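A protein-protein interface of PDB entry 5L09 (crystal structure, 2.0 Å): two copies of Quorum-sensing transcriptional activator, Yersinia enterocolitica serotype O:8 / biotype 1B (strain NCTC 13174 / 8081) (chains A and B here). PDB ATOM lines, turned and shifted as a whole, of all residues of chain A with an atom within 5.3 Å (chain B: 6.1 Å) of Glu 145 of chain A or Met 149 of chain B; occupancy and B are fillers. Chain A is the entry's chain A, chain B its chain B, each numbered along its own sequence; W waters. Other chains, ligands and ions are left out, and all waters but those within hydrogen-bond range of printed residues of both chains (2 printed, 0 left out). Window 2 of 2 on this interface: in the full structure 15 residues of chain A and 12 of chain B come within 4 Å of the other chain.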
ATOM      1  N   PRO A  79     -24.594  24.282   4.289  1.00  0.00           N
ATOM      2  CA  PRO A  79     -24.332  22.863   4.547  1.00  0.00           C
ATOM      3  C   PRO A  79     -25.620  22.058   4.554  1.00  0.00           C
ATOM      4  O   PRO A  79     -26.699  22.570   4.869  1.00  0.00           O
ATOM      5  CB  PRO A  79     -23.686  22.860   5.936  1.00  0.00           C
ATOM      6  CG  PRO A  79     -23.523  24.277   6.337  1.00  0.00           C
ATOM      7  CD  PRO A  79     -24.354  25.124   5.471  1.00  0.00           C
ATOM      8  N   GLU A 141     -24.671  19.506  14.373  1.00  0.00           N
ATOM      9  CA  GLU A 141     -25.717  20.517  14.393  1.00  0.00           C
ATOM     10  C   GLU A 141     -25.315  21.706  15.255  1.00  0.00           C
ATOM     11  O   GLU A 141     -25.573  22.857  14.889  1.00  0.00           O
ATOM     12  CB  GLU A 141     -27.041  19.928  14.894  1.00  0.00           C
ATOM     13  CG  GLU A 141     -27.650  18.892  13.937  1.00  0.00           C
ATOM     14  CD  GLU A 141     -28.052  19.495  12.592  1.00  0.00           C
ATOM     15  OE1 GLU A 141     -28.343  20.706  12.557  1.00  0.00           O
ATOM     16  OE2 GLU A 141     -28.102  18.753  11.584  1.00  0.00           O
ATOM     17  N   ILE A 142     -24.690  21.460  16.400  1.00  0.00           N
ATOM     18  CA  ILE A 142     -24.373  22.618  17.238  1.00  0.00           C
ATOM     19  C   ILE A 142     -23.087  23.304  16.779  1.00  0.00           C
ATOM     20  O   ILE A 142     -22.876  24.476  17.106  1.00  0.00           O
ATOM     21  CB  ILE A 142     -24.268  22.257  18.729  1.00  0.00           C
ATOM     22  CG1 ILE A 142     -23.063  21.366  18.998  1.00  0.00           C
ATOM     23  CG2 ILE A 142     -25.554  21.626  19.228  1.00  0.00           C
ATOM     24  CD1 ILE A 142     -22.104  21.991  19.973  1.00  0.00           C
ATOM     25  N   ASN A 143     -22.233  22.622  16.012  1.00  0.00           N
ATOM     26  CA  ASN A 143     -20.946  23.178  15.599  1.00  0.00           C
ATOM     27  C   ASN A 143     -20.887  23.542  14.123  1.00  0.00           C
ATOM     28  O   ASN A 143     -19.791  23.784  13.600  1.00  0.00           O
ATOM     29  CB  ASN A 143     -19.824  22.194  15.919  1.00  0.00           C
ATOM     30  CG  ASN A 143     -19.583  22.067  17.405  1.00  0.00           C
ATOM     31  OD1 ASN A 143     -19.195  23.029  18.056  1.00  0.00           O
ATOM     32  ND2 ASN A 143     -19.806  20.876  17.947  1.00  0.00           N
ATOM     33  N   LYS A 144     -22.026  23.601  13.438  1.00  0.00           N
ATOM     34  CA  LYS A 144     -21.989  23.758  11.985  1.00  0.00           C
ATOM     35  C   LYS A 144     -21.349  25.079  11.559  1.00  0.00           C
ATOM     36  O   LYS A 144     -20.697  25.131  10.517  1.00  0.00           O
ATOM     37  CB  LYS A 144     -23.394  23.635  11.397  1.00  0.00           C
ATOM     38  CG  LYS A 144     -24.386  24.633  11.900  1.00  0.00           C
ATOM     39  CD  LYS A 144     -25.752  24.391  11.264  1.00  0.00           C
ATOM     40  CE  LYS A 144     -26.863  25.131  12.007  1.00  0.00           C
ATOM     41  NZ  LYS A 144     -26.713  26.622  12.009  1.00  0.00           N
ATOM     42  N   GLU A 145     -21.518  26.148  12.338  1.00  0.00           N
ATOM     43  CA  GLU A 145     -20.876  27.409  11.971  1.00  0.00           C
ATOM     44  C   GLU A 145     -19.357  27.308  12.071  1.00  0.00           C
ATOM     45  O   GLU A 145     -18.634  27.886  11.247  1.00  0.00           O
ATOM     46  CB  GLU A 145     -21.398  28.550  12.849  1.00  0.00           C
ATOM     47  CG  GLU A 145     -22.880  28.839  12.659  1.00  0.00           C
ATOM     48  CD  GLU A 145     -23.774  27.849  13.389  1.00  0.00           C
ATOM     49  OE1 GLU A 145     -24.952  27.714  12.990  1.00  0.00           O
ATOM     50  OE2 GLU A 145     -23.300  27.187  14.343  1.00  0.00           O
ATOM     51  N   LYS A 146     -18.852  26.591  13.076  1.00  0.00           N
ATOM     52  CA  LYS A 146     -17.409  26.435  13.208  1.00  0.00           C
ATOM     53  C   LYS A 146     -16.840  25.516  12.138  1.00  0.00           C
ATOM     54  O   LYS A 146     -15.693  25.697  11.705  1.00  0.00           O
ATOM     55  CB  LYS A 146     -17.066  25.886  14.594  1.00  0.00           C
ATOM     56  CG  LYS A 146     -17.445  26.850  15.750  1.00  0.00           C
ATOM     57  CD  LYS A 146     -17.284  26.175  17.105  1.00  0.00           C
ATOM     58  CE  LYS A 146     -18.080  26.932  18.178  1.00  0.00           C
ATOM     59  NZ  LYS A 146     -17.434  26.883  19.519  1.00  0.00           N
ATOM     60  N   ILE A 147     -17.599  24.505  11.737  1.00  0.00           N
ATOM     61  CA  ILE A 147     -17.117  23.579  10.718  1.00  0.00           C
ATOM     62  C   ILE A 147     -17.075  24.266   9.359  1.00  0.00           C
ATOM     63  O   ILE A 147     -16.121  24.098   8.585  1.00  0.00           O
ATOM     64  CB  ILE A 147     -18.004  22.317  10.710  1.00  0.00           C
ATOM     65  CG1 ILE A 147     -17.837  21.573  12.048  1.00  0.00           C
ATOM     66  CG2 ILE A 147     -17.599  21.394   9.554  1.00  0.00           C
ATOM     67  CD1 ILE A 147     -18.706  20.340  12.224  1.00  0.00           C
ATOM     68  N   GLN A 148     -18.098  25.066   9.052  1.00  0.00           N
ATOM     69  CA  GLN A 148     -18.047  25.869   7.836  1.00  0.00           C
ATOM     70  C   GLN A 148     -16.822  26.772   7.828  1.00  0.00           C
ATOM     71  O   GLN A 148     -16.158  26.913   6.795  1.00  0.00           O
ATOM     72  CB  GLN A 148     -19.316  26.710   7.683  1.00  0.00           C
ATOM     73  CG  GLN A 148     -19.272  27.620   6.426  1.00  0.00           C
ATOM     74  CD  GLN A 148     -19.463  26.828   5.134  1.00  0.00           C
ATOM     75  OE1 GLN A 148     -19.994  25.718   5.150  1.00  0.00           O
ATOM     76  NE2 GLN A 148     -19.064  27.417   3.998  1.00  0.00           N
ATOM     77  N   MET A 149     -16.496  27.387   8.970  1.00  0.00           N
ATOM     78  CA  MET A 149     -15.339  28.267   9.002  1.00  0.00           C
ATOM     79  C   MET A 149     -14.053  27.447   8.821  1.00  0.00           C
ATOM     80  O   MET A 149     -13.115  27.919   8.199  1.00  0.00           O
ATOM     81  CB  MET A 149     -15.284  29.082  10.316  1.00  0.00           C
ATOM     82  CG  MET A 149     -14.165  30.146  10.344  1.00  0.00           C
ATOM     83  SD  MET A 149     -14.229  31.482   8.856  1.00  0.00           S
ATOM     84  CE  MET A 149     -15.960  32.297   9.169  1.00  0.00           C
ATOM     85  N   LEU A 150     -14.013  26.221   9.364  1.00  0.00           N
ATOM     86  CA  LEU A 150     -12.859  25.362   9.103  1.00  0.00           C
ATOM     87  C   LEU A 150     -12.666  25.128   7.602  1.00  0.00           C
ATOM     88  O   LEU A 150     -11.539  25.198   7.091  1.00  0.00           O
ATOM     89  CB  LEU A 150     -12.999  24.025   9.850  1.00  0.00           C
ATOM     90  CG  LEU A 150     -11.892  23.002   9.540  1.00  0.00           C
ATOM     91  CD1 LEU A 150     -10.498  23.570   9.886  1.00  0.00           C
ATOM     92  CD2 LEU A 150     -12.114  21.687  10.293  1.00  0.00           C
ATOM     93  N   LYS B 144     -17.532  35.748  14.458  1.00  0.00           N
ATOM     94  CA  LYS B 144     -17.372  35.775  13.003  1.00  0.00           C
ATOM     95  C   LYS B 144     -17.952  34.525  12.329  1.00  0.00           C
ATOM     96  O   LYS B 144     -18.537  34.625  11.245  1.00  0.00           O
ATOM     97  CB  LYS B 144     -15.903  35.966  12.628  1.00  0.00           C
ATOM     98  CG  LYS B 144     -14.973  34.839  13.018  1.00  0.00           C
ATOM     99  CD  LYS B 144     -13.519  35.196  12.699  1.00  0.00           C
ATOM    100  CE  LYS B 144     -13.234  35.120  11.200  1.00  0.00           C
ATOM    101  NZ  LYS B 144     -11.748  35.204  10.922  1.00  0.00           N
ATOM    102  N   GLU B 145     -17.802  33.336  12.945  1.00  0.00           N
ATOM    103  CA  GLU B 145     -18.372  32.125  12.349  1.00  0.00           C
ATOM    104  C   GLU B 145     -19.883  32.224  12.244  1.00  0.00           C
ATOM    105  O   GLU B 145     -20.481  31.784  11.251  1.00  0.00           O
ATOM    106  CB  GLU B 145     -18.002  30.878  13.158  1.00  0.00           C
ATOM    107  CG  GLU B 145     -16.533  30.575  13.212  1.00  0.00           C
ATOM    108  CD  GLU B 145     -15.769  31.471  14.168  1.00  0.00           C
ATOM    109  OE1 GLU B 145     -16.409  32.105  15.046  1.00  0.00           O
ATOM    110  OE2 GLU B 145     -14.526  31.539  14.033  1.00  0.00           O
ATOM    111  N   LYS B 146     -20.527  32.786  13.269  1.00  0.00           N
ATOM    112  CA  LYS B 146     -21.976  32.925  13.236  1.00  0.00           C
ATOM    113  C   LYS B 146     -22.418  33.947  12.199  1.00  0.00           C
ATOM    114  O   LYS B 146     -23.463  33.784  11.557  1.00  0.00           O
ATOM    115  CB  LYS B 146     -22.495  33.318  14.629  1.00  0.00           C
ATOM    116  CG  LYS B 146     -22.465  32.165  15.621  1.00  0.00           C
ATOM    117  CD  LYS B 146     -22.800  32.642  17.043  1.00  0.00           C
ATOM    118  CE  LYS B 146     -22.458  31.579  18.082  1.00  0.00           C
ATOM    119  NZ  LYS B 146     -22.838  32.004  19.460  1.00  0.00           N
ATOM    120  N   ILE B 147     -21.659  35.030  12.046  1.00  0.00           N
ATOM    121  CA  ILE B 147     -22.037  36.040  11.066  1.00  0.00           C
ATOM    122  C   ILE B 147     -21.836  35.501   9.651  1.00  0.00           C
ATOM    123  O   ILE B 147     -22.631  35.783   8.743  1.00  0.00           O
ATOM    124  CB  ILE B 147     -21.242  37.333  11.329  1.00  0.00           C
ATOM    125  CG1 ILE B 147     -21.691  37.922  12.683  1.00  0.00           C
ATOM    126  CG2 ILE B 147     -21.434  38.324  10.185  1.00  0.00           C
ATOM    127  CD1 ILE B 147     -20.854  39.067  13.164  1.00  0.00           C
ATOM    128  N   GLN B 148     -20.786  34.699   9.446  1.00  0.00           N
ATOM    129  CA  GLN B 148     -20.617  34.060   8.135  1.00  0.00           C
ATOM    130  C   GLN B 148     -21.806  33.166   7.809  1.00  0.00           C
ATOM    131  O   GLN B 148     -22.322  33.172   6.681  1.00  0.00           O
ATOM    132  CB  GLN B 148     -19.318  33.258   8.103  1.00  0.00           C
ATOM    133  CG  GLN B 148     -19.067  32.553   6.768  1.00  0.00           C
ATOM    134  CD  GLN B 148     -18.724  33.524   5.635  1.00  0.00           C
ATOM    135  OE1 GLN B 148     -18.253  34.645   5.874  1.00  0.00           O
ATOM    136  NE2 GLN B 148     -18.937  33.081   4.392  1.00  0.00           N
ATOM    137  N   MET B 149     -22.281  32.413   8.790  1.00  0.00           N
ATOM    138  CA  MET B 149     -23.444  31.571   8.560  1.00  0.00           C
ATOM    139  C   MET B 149     -24.694  32.378   8.278  1.00  0.00           C
ATOM    140  O   MET B 149     -25.545  31.941   7.497  1.00  0.00           O
ATOM    141  CB  MET B 149     -23.691  30.640   9.751  1.00  0.00           C
ATOM    142  CG  MET B 149     -24.782  29.588   9.455  1.00  0.00           C
ATOM    143  SD  MET B 149     -24.373  28.403   7.894  1.00  0.00           S
ATOM    144  CE  MET B 149     -22.649  27.737   8.396  1.00  0.00           C
ATOM    145  N   LEU B 150     -24.829  33.551   8.914  1.00  0.00           N
ATOM    146  CA  LEU B 150     -25.970  34.409   8.591  1.00  0.00           C
ATOM    147  C   LEU B 150     -25.923  34.868   7.140  1.00  0.00           C
ATOM    148  O   LEU B 150     -26.953  34.904   6.459  1.00  0.00           O
ATOM    149  CB  LEU B 150     -26.012  35.624   9.520  1.00  0.00           C
ATOM    150  CG  LEU B 150     -27.077  36.699   9.234  1.00  0.00           C
ATOM    151  CD1 LEU B 150     -28.496  36.147   9.442  1.00  0.00           C
ATOM    152  CD2 LEU B 150     -26.851  37.947  10.087  1.00  0.00           C
ATOM    153  N   LEU B 151     -24.737  35.234   6.642  1.00  0.00           N
ATOM    154  CA  LEU B 151     -24.632  35.556   5.222  1.00  0.00           C
ATOM    155  C   LEU B 151     -25.015  34.357   4.366  1.00  0.00           C
ATOM    156  O   LEU B 151     -25.751  34.491   3.378  1.00  0.00           O
ATOM    157  CB  LEU B 151     -23.208  36.015   4.885  1.00  0.00           C
ATOM    158  CG  LEU B 151     -22.813  36.116   3.404  1.00  0.00           C
ATOM    159  CD1 LEU B 151     -23.701  37.156   2.681  1.00  0.00           C
ATOM    160  CD2 LEU B 151     -21.299  36.488   3.273  1.00  0.00           C
ATOM    161  N   ILE B 152     -24.493  33.174   4.711  1.00  0.00           N
ATOM    162  CA  ILE B 152     -24.780  31.968   3.932  1.00  0.00           C
ATOM    163  C   ILE B 152     -26.287  31.686   3.915  1.00  0.00           C
ATOM    164  O   ILE B 152     -26.874  31.381   2.867  1.00  0.00           O
ATOM    165  CB  ILE B 152     -23.997  30.768   4.494  1.00  0.00           C
ATOM    166  CG1 ILE B 152     -22.501  30.869   4.160  1.00  0.00           C
ATOM    167  CG2 ILE B 152     -24.564  29.439   3.942  1.00  0.00           C
ATOM    168  CD1 ILE B 152     -21.638  29.933   5.021  1.00  0.00           C
ATOM    169  N   LEU B 153     -26.927  31.761   5.081  1.00  0.00           N
ATOM    170  CA  LEU B 153     -28.351  31.411   5.150  1.00  0.00           C
ATOM    171  C   LEU B 153     -29.231  32.514   4.582  1.00  0.00           C
ATOM    172  O   LEU B 153     -30.270  32.220   3.979  1.00  0.00           O
ATOM    173  CB  LEU B 153     -28.758  31.082   6.594  1.00  0.00           C
ATOM    174  CG  LEU B 153     -28.103  29.855   7.249  1.00  0.00           C
ATOM    175  CD1 LEU B 153     -28.530  29.723   8.713  1.00  0.00           C
ATOM    176  CD2 LEU B 153     -28.399  28.560   6.484  1.00  0.00           C
ATOM    177  N   THR B 154     -28.831  33.779   4.730  1.00  0.00           N
ATOM    178  CA  THR B 154     -29.535  34.849   4.027  1.00  0.00           C
ATOM    179  C   THR B 154     -29.498  34.616   2.525  1.00  0.00           C
ATOM    180  O   THR B 154     -30.523  34.692   1.838  1.00  0.00           O
ATOM    181  CB  THR B 154     -28.911  36.206   4.367  1.00  0.00           C
ATOM    182  OG1 THR B 154     -29.060  36.469   5.764  1.00  0.00           O
ATOM    183  CG2 THR B 154     -29.562  37.341   3.561  1.00  0.00           C
HETATM  184  O   HOH W   1     -18.957  30.242   2.807  1.00  0.00           O
HETATM  185  O   HOH W   2     -19.398  29.865   9.481  1.00  0.00           O
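O of Lys 144 of chain A touches CE of Met 149 of chain B (3.9 Å). Glu 145 of chain A touches Glu 145 of chain B (O to CB, 3.6 Å). CB of Met 149 of chain B touches CG of Glu 145 of chain A (3.5 Å). Met 149 of chain B touches Gln 148 of chain A. Gln 148 of chain A touches Ile 152 of chain B. Met 149 of chain A touches Glu 145 of chain B. CE of Met 149 of chain A touches CB of Gln 148 of chain B, 3.7 Å away.
Of the 11 printed residues of chain A, 4 touch a printed residue of chain B. Hydrophobic or aromatic side chains of chain A within 4 Å of the printed part of chain B: Met 149. Hydrophobic or aromatic side chains of chain B that line the printed part of chain A: Met 149 and Ile 152. Among the printed residues, 7 pairs touch across the chains. Among the printed residues, no Asp or Glu carboxylate lies within 4 Å of a Lys or Arg side-chain nitrogen of the other chain.
Lys 144 of chain A touches Met 149 of chain B, but with the chains exchanged Met 149 of chain A does not touch Lys 144 of chain B (4.05 Å). Glu 145 of chain B touches its own counterpart, Glu 145 of chain A. Glu 145 of chain A touches Met 149 of chain B, and with the chains exchanged Met 149 of chain A touches Glu 145 of chain B. Gln 148 of chain A touches Met 149 of chain B, and with the chains exchanged Met 149 of chain A touches Gln 148 of chain B. Of the 7 pairs that touch across the chains among the printed residues, 5 have their exchanged pair printed and touching as well.
Water W2 bridges O of Glu 145 of chain A and O of Glu 145 of chain B. Water W1 bridges NE2 of Gln 148 of chain A (3.1 Å) and NE2 of Gln 148 of chain B (3.3 Å).
Glu 141 of chain A touches none of the printed residues of chain B. Asn 143 of chain A touches none of the printed residues of chain B. Printed residues of chain B within 4 Å of Glu 145 of chain A: Glu 145 (3.6 Å) and Met 149 (3.5 Å). Of the printed residues of chain A, Glu 145 of chain B touches Glu 145 (3.6 Å) and Met 149 (3.5 Å). Printed residues of chain A within 4 Å of Gln 148 of chain B: Met 149. Of the printed residues of chain A, Met 149 of chain B touches Lys 144, Glu 145 and Gln 148. Of the printed residues of chain A, Ile 152 of chain B touches Gln 148. The nearest printed residue of chain B that does not touch Glu 145 of chain A is Lys 146 of chain B (4.2 Å). The nearest printed residue of chain B that does not touch Gln 148 of chain A is Gln 148 of chain B (4.9 Å).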
